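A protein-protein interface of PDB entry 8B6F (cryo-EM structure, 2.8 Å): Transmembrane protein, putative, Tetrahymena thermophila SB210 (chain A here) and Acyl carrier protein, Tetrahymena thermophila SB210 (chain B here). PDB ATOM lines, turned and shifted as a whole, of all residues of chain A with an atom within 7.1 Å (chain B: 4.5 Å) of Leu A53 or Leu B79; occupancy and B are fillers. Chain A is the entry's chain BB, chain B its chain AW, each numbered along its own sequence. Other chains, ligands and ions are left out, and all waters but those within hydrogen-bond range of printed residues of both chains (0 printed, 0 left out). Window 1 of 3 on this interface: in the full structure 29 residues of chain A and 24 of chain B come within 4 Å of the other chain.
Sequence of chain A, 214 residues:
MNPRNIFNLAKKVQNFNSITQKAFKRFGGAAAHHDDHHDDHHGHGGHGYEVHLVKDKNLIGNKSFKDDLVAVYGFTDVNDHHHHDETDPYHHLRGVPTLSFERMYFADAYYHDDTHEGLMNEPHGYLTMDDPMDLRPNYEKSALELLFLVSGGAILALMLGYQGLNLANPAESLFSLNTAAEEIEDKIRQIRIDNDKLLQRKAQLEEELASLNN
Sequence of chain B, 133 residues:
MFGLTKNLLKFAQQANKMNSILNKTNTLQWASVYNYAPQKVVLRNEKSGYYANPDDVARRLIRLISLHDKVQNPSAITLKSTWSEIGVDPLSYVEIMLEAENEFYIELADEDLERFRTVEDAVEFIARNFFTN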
ATOM      1  N   GLU A  50      32.747  22.627   4.975  1.00  0.00           N
ATOM      2  CA  GLU A  50      31.313  22.859   5.057  1.00  0.00           C
ATOM      3  C   GLU A  50      30.710  22.003   6.164  1.00  0.00           C
ATOM      4  O   GLU A  50      31.116  20.857   6.377  1.00  0.00           O
ATOM      5  CB  GLU A  50      30.649  22.555   3.712  1.00  0.00           C
ATOM      6  CG  GLU A  50      30.843  21.127   3.204  1.00  0.00           C
ATOM      7  CD  GLU A  50      29.798  20.156   3.726  1.00  0.00           C
ATOM      8  OE1 GLU A  50      28.853  20.599   4.412  1.00  0.00           O
ATOM      9  OE2 GLU A  50      29.919  18.946   3.441  1.00  0.00           O
ATOM     10  N   VAL A  51      29.737  22.567   6.874  1.00  0.00           N
ATOM     11  CA  VAL A  51      29.123  21.928   8.031  1.00  0.00           C
ATOM     12  C   VAL A  51      27.721  21.471   7.659  1.00  0.00           C
ATOM     13  O   VAL A  51      26.970  22.204   7.005  1.00  0.00           O
ATOM     14  CB  VAL A  51      29.087  22.874   9.248  1.00  0.00           C
ATOM     15  CG1 VAL A  51      30.494  23.310   9.621  1.00  0.00           C
ATOM     16  CG2 VAL A  51      28.209  24.088   8.964  1.00  0.00           C
ATOM     17  N   HIS A  52      27.374  20.255   8.071  1.00  0.00           N
ATOM     18  CA  HIS A  52      26.041  19.703   7.844  1.00  0.00           C
ATOM     19  C   HIS A  52      25.138  20.178   8.976  1.00  0.00           C
ATOM     20  O   HIS A  52      25.137  19.606  10.068  1.00  0.00           O
ATOM     21  CB  HIS A  52      26.093  18.182   7.771  1.00  0.00           C
ATOM     22  CG  HIS A  52      24.752  17.539   7.597  1.00  0.00           C
ATOM     23  ND1 HIS A  52      23.838  17.434   8.623  1.00  0.00           N
ATOM     24  CD2 HIS A  52      24.175  16.962   6.517  1.00  0.00           C
ATOM     25  CE1 HIS A  52      22.753  16.823   8.182  1.00  0.00           C
ATOM     26  NE2 HIS A  52      22.931  16.526   6.907  1.00  0.00           N
ATOM     27  N   LEU A  53      24.365  21.230   8.715  1.00  0.00           N
ATOM     28  CA  LEU A  53      23.434  21.788   9.687  1.00  0.00           C
ATOM     29  C   LEU A  53      22.052  21.855   9.058  1.00  0.00           C
ATOM     30  O   LEU A  53      21.903  22.350   7.936  1.00  0.00           O
ATOM     31  CB  LEU A  53      23.882  23.179  10.151  1.00  0.00           C
ATOM     32  CG  LEU A  53      23.003  23.864  11.201  1.00  0.00           C
ATOM     33  CD1 LEU A  53      22.891  23.021  12.464  1.00  0.00           C
ATOM     34  CD2 LEU A  53      23.549  25.244  11.531  1.00  0.00           C
ATOM     35  N   VAL A  54      21.049  21.359   9.777  1.00  0.00           N
ATOM     36  CA  VAL A  54      19.679  21.291   9.285  1.00  0.00           C
ATOM     37  C   VAL A  54      18.920  22.512   9.784  1.00  0.00           C
ATOM     38  O   VAL A  54      18.873  22.775  10.992  1.00  0.00           O
ATOM     39  CB  VAL A  54      18.989  19.992   9.738  1.00  0.00           C
ATOM     40  CG1 VAL A  54      17.525  19.977   9.314  1.00  0.00           C
ATOM     41  CG2 VAL A  54      19.718  18.784   9.175  1.00  0.00           C
ATOM     42  N   LYS A  55      18.323  23.254   8.855  1.00  0.00           N
ATOM     43  CA  LYS A  55      17.518  24.422   9.172  1.00  0.00           C
ATOM     44  C   LYS A  55      16.170  24.295   8.479  1.00  0.00           C
ATOM     45  O   LYS A  55      16.047  23.635   7.443  1.00  0.00           O
ATOM     46  CB  LYS A  55      18.210  25.721   8.738  1.00  0.00           C
ATOM     47  CG  LYS A  55      19.603  25.897   9.317  1.00  0.00           C
ATOM     48  CD  LYS A  55      20.203  27.237   8.931  1.00  0.00           C
ATOM     49  CE  LYS A  55      21.590  27.403   9.528  1.00  0.00           C
ATOM     50  NZ  LYS A  55      22.148  28.758   9.272  1.00  0.00           N
ATOM     51  N   ASP A  56      15.157  24.929   9.065  1.00  0.00           N
ATOM     52  CA  ASP A  56      13.772  24.911   8.606  1.00  0.00           C
ATOM     53  C   ASP A  56      13.087  23.574   8.860  1.00  0.00           C
ATOM     54  O   ASP A  56      11.929  23.406   8.460  1.00  0.00           O
ATOM     55  CB  ASP A  56      13.646  25.239   7.109  1.00  0.00           C
ATOM     56  CG  ASP A  56      14.260  26.578   6.752  1.00  0.00           C
ATOM     57  OD1 ASP A  56      14.020  27.558   7.486  1.00  0.00           O
ATOM     58  OD2 ASP A  56      14.987  26.649   5.740  1.00  0.00           O
ATOM     59  N   LYS A  57      13.752  22.620   9.508  1.00  0.00           N
ATOM     60  CA  LYS A  57      13.178  21.313   9.784  1.00  0.00           C
ATOM     61  C   LYS A  57      13.388  20.964  11.250  1.00  0.00           C
ATOM     62  O   LYS A  57      14.400  21.328  11.852  1.00  0.00           O
ATOM     63  CB  LYS A  57      13.803  20.230   8.895  1.00  0.00           C
ATOM     64  CG  LYS A  57      13.744  20.551   7.411  1.00  0.00           C
ATOM     65  CD  LYS A  57      14.456  19.498   6.571  1.00  0.00           C
ATOM     66  CE  LYS A  57      13.715  18.170   6.583  1.00  0.00           C
ATOM     67  NZ  LYS A  57      14.345  17.175   5.669  1.00  0.00           N
ATOM     68  N   ASN A  58      12.420  20.252  11.816  1.00  0.00           N
ATOM     69  CA  ASN A  58      12.497  19.866  13.217  1.00  0.00           C
ATOM     70  C   ASN A  58      13.624  18.863  13.434  1.00  0.00           C
ATOM     71  O   ASN A  58      14.000  18.114  12.529  1.00  0.00           O
ATOM     72  CB  ASN A  58      11.170  19.269  13.682  1.00  0.00           C
ATOM     73  CG  ASN A  58      10.827  17.979  12.964  1.00  0.00           C
ATOM     74  OD1 ASN A  58      11.191  17.783  11.805  1.00  0.00           O
ATOM     75  ND2 ASN A  58      10.122  17.089  13.652  1.00  0.00           N
ATOM     76  N   LEU A  59      14.171  18.858  14.653  1.00  0.00           N
ATOM     77  CA  LEU A  59      15.241  17.938  15.009  1.00  0.00           C
ATOM     78  C   LEU A  59      14.816  16.866  16.003  1.00  0.00           C
ATOM     79  O   LEU A  59      15.477  15.826  16.081  1.00  0.00           O
ATOM     80  CB  LEU A  59      16.450  18.700  15.578  1.00  0.00           C
ATOM     81  CG  LEU A  59      17.009  19.836  14.709  1.00  0.00           C
ATOM     82  CD1 LEU A  59      18.322  20.371  15.260  1.00  0.00           C
ATOM     83  CD2 LEU A  59      17.198  19.400  13.272  1.00  0.00           C
ATOM     84  N   PRO B  54      28.142  22.222  15.444  1.00  0.00           N
ATOM     85  CA  PRO B  54      26.889  22.989  15.523  1.00  0.00           C
ATOM     86  C   PRO B  54      25.653  22.114  15.556  1.00  0.00           C
ATOM     87  O   PRO B  54      24.665  22.480  16.205  1.00  0.00           O
ATOM     88  CB  PRO B  54      26.934  23.867  14.266  1.00  0.00           C
ATOM     89  CG  PRO B  54      27.834  23.158  13.336  1.00  0.00           C
ATOM     90  CD  PRO B  54      28.858  22.477  14.182  1.00  0.00           C
ATOM     91  N   ASP B  55      25.670  20.969  14.873  1.00  0.00           N
ATOM     92  CA  ASP B  55      24.514  20.080  14.905  1.00  0.00           C
ATOM     93  C   ASP B  55      24.270  19.564  16.317  1.00  0.00           C
ATOM     94  O   ASP B  55      23.137  19.576  16.809  1.00  0.00           O
ATOM     95  CB  ASP B  55      24.722  18.921  13.931  1.00  0.00           C
ATOM     96  CG  ASP B  55      23.445  18.156  13.653  1.00  0.00           C
ATOM     97  OD1 ASP B  55      22.535  18.182  14.507  1.00  0.00           O
ATOM     98  OD2 ASP B  55      23.349  17.529  12.578  1.00  0.00           O
ATOM     99  N   ALA B  58      22.964  22.408  18.499  1.00  0.00           N
ATOM    100  CA  ALA B  58      21.556  22.693  18.248  1.00  0.00           C
ATOM    101  C   ALA B  58      20.654  21.628  18.856  1.00  0.00           C
ATOM    102  O   ALA B  58      19.619  21.950  19.452  1.00  0.00           O
ATOM    103  CB  ALA B  58      21.307  22.801  16.746  1.00  0.00           C
ATOM    104  N   THR B  78      12.276  24.618  15.615  1.00  0.00           N
ATOM    105  CA  THR B  78      13.294  24.599  14.577  1.00  0.00           C
ATOM    106  C   THR B  78      14.258  25.748  14.831  1.00  0.00           C
ATOM    107  O   THR B  78      13.985  26.652  15.624  1.00  0.00           O
ATOM    108  CB  THR B  78      12.690  24.711  13.172  1.00  0.00           C
ATOM    109  OG1 THR B  78      12.041  25.980  13.023  1.00  0.00           O
ATOM    110  CG2 THR B  78      11.683  23.600  12.931  1.00  0.00           C
ATOM    111  N   LEU B  79      15.401  25.708  14.146  1.00  0.00           N
ATOM    112  CA  LEU B  79      16.399  26.755  14.328  1.00  0.00           C
ATOM    113  C   LEU B  79      15.856  28.124  13.946  1.00  0.00           C
ATOM    114  O   LEU B  79      16.288  29.139  14.504  1.00  0.00           O
ATOM    115  CB  LEU B  79      17.652  26.435  13.514  1.00  0.00           C
ATOM    116  CG  LEU B  79      18.473  25.239  13.999  1.00  0.00           C
ATOM    117  CD1 LEU B  79      19.663  24.994  13.092  1.00  0.00           C
ATOM    118  CD2 LEU B  79      18.929  25.437  15.433  1.00  0.00           C
ATOM    119  N   LYS B  80      14.911  28.175  13.015  1.00  0.00           N
ATOM    120  CA  LYS B  80      14.327  29.432  12.567  1.00  0.00           C
ATOM    121  C   LYS B  80      13.114  29.848  13.386  1.00  0.00           C
ATOM    122  O   LYS B  80      12.493  30.866  13.067  1.00  0.00           O
ATOM    123  CB  LYS B  80      13.935  29.330  11.090  1.00  0.00           C
ATOM    124  CG  LYS B  80      15.105  29.072  10.152  1.00  0.00           C
ATOM    125  CD  LYS B  80      16.087  30.236  10.144  1.00  0.00           C
ATOM    126  CE  LYS B  80      17.213  30.008   9.149  1.00  0.00           C
ATOM    127  NZ  LYS B  80      16.714  29.877   7.751  1.00  0.00           N
ATOM    128  N   SER B  81      12.759  29.091  14.420  1.00  0.00           N
ATOM    129  CA  SER B  81      11.591  29.393  15.233  1.00  0.00           C
ATOM    130  C   SER B  81      11.964  30.391  16.322  1.00  0.00           C
ATOM    131  O   SER B  81      12.975  30.220  17.009  1.00  0.00           O
ATOM    132  CB  SER B  81      11.022  28.120  15.861  1.00  0.00           C
ATOM    133  OG  SER B  81      10.708  27.156  14.872  1.00  0.00           O
ATOM    134  N   THR B 118      16.441  34.088  17.755  1.00  0.00           N
ATOM    135  CA  THR B 118      15.935  32.792  17.333  1.00  0.00           C
ATOM    136  C   THR B 118      16.886  31.708  17.810  1.00  0.00           C
ATOM    137  O   THR B 118      18.033  31.974  18.179  1.00  0.00           O
ATOM    138  CB  THR B 118      15.776  32.705  15.809  1.00  0.00           C
ATOM    139  OG1 THR B 118      17.010  33.054  15.169  1.00  0.00           O
ATOM    140  CG2 THR B 118      14.680  33.631  15.328  1.00  0.00           C
ATOM    141  N   VAL B 119      16.388  30.471  17.802  1.00  0.00           N
ATOM    142  CA  VAL B 119      17.233  29.332  18.141  1.00  0.00           C
ATOM    143  C   VAL B 119      18.421  29.265  17.196  1.00  0.00           C
ATOM    144  O   VAL B 119      19.509  28.824  17.584  1.00  0.00           O
ATOM    145  CB  VAL B 119      16.414  28.026  18.116  1.00  0.00           C
ATOM    146  CG1 VAL B 119      17.278  26.845  18.536  1.00  0.00           C
ATOM    147  CG2 VAL B 119      15.194  28.140  19.015  1.00  0.00           C
ATOM    148  N   GLU B 120      18.243  29.709  15.952  1.00  0.00           N
ATOM    149  CA  GLU B 120      19.360  29.771  15.016  1.00  0.00           C
ATOM    150  C   GLU B 120      20.473  30.655  15.562  1.00  0.00           C
ATOM    151  O   GLU B 120      21.641  30.253  15.598  1.00  0.00           O
ATOM    152  CB  GLU B 120      18.870  30.291  13.662  1.00  0.00           C
ATOM    153  CG  GLU B 120      19.969  30.590  12.652  1.00  0.00           C
ATOM    154  CD  GLU B 120      20.758  29.358  12.267  1.00  0.00           C
ATOM    155  OE1 GLU B 120      20.336  28.242  12.635  1.00  0.00           O
ATOM    156  OE2 GLU B 120      21.799  29.505  11.593  1.00  0.00           O
ATOM    157  N   VAL B 123      22.157  28.983  18.738  1.00  0.00           N
ATOM    158  CA  VAL B 123      23.070  27.879  18.458  1.00  0.00           C
ATOM    159  C   VAL B 123      24.310  28.380  17.732  1.00  0.00           C
ATOM    160  O   VAL B 123      25.422  27.897  17.973  1.00  0.00           O
ATOM    161  CB  VAL B 123      22.361  26.771  17.656  1.00  0.00           C
ATOM    162  CG1 VAL B 123      21.151  26.254  18.417  1.00  0.00           C
ATOM    163  CG2 VAL B 123      21.970  27.259  16.271  1.00  0.00           C
ATOM    164  N   GLU B 124      24.146  29.352  16.833  1.00  0.00           N
ATOM    165  CA  GLU B 124      25.303  29.905  16.139  1.00  0.00           C
ATOM    166  C   GLU B 124      26.278  30.532  17.125  1.00  0.00           C
ATOM    167  O   GLU B 124      27.486  30.288  17.059  1.00  0.00           O
ATOM    168  CB  GLU B 124      24.850  30.933  15.102  1.00  0.00           C
ATOM    169  CG  GLU B 124      24.248  30.319  13.847  1.00  0.00           C
ATOM    170  CD  GLU B 124      25.266  29.556  13.023  1.00  0.00           C
ATOM    171  OE1 GLU B 124      26.463  29.906  13.084  1.00  0.00           O
ATOM    172  OE2 GLU B 124      24.874  28.604  12.316  1.00  0.00           O
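The side-chain amino group of Lys B80 lies within salt-bridge range of the side-chain carboxylate of Asp A56, at 3.6 Å. OE2 of Glu B120 is in salt-bridge range of NZ of Lys A55 (2.5 Å).
OG1 of Thr B78 lies within hydrogen-bond range of OG of Ser B81 (2.6 Å). O of Leu B79 lies within hydrogen-bond range of N of Glu B120 (2.5 Å).
O of His A52 touches OD2 of Asp B55, 3.7 Å away. Leu A53 touches Leu B79. Glu B124 touches Leu A53 (OE2 to CD2, 3.7 Å). Leu B79 touches Val A54 (CD1 to O, 3.2 Å). Lys A55 touches Leu B79. Thr B78 touches Lys A57. Thr B78 touches Asn A58.
Leu A53 touches just these residues of chain B: Leu B79 and Glu B124. Of the printed residues of chain B, Lys A57 touches Thr B78. Leu B79 touches just these residues of chain A: Leu A53, Val A54 and Lys A55. Of the printed residues of chain A, Glu B120 touches Lys A55. The nearest printed residue of chain A that does not touch Leu B79 is Leu A59 (5.0 Å).
Hydrophobic or aromatic side chains of chain B within 4 Å of the printed part of chain A: Leu B79. Of the 10 printed residues of chain A, 7 touch a printed residue of chain B. Hydrophobic or aromatic side chains of chain A within 4 Å of the printed part of chain B: His A52 and Leu A53. Among the printed residues, Asp or Glu carboxylates within 4 Å of a Lys or Arg side-chain nitrogen of the other chain: Lys A55 with Glu B120 and Asp A56 with Lys B80.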
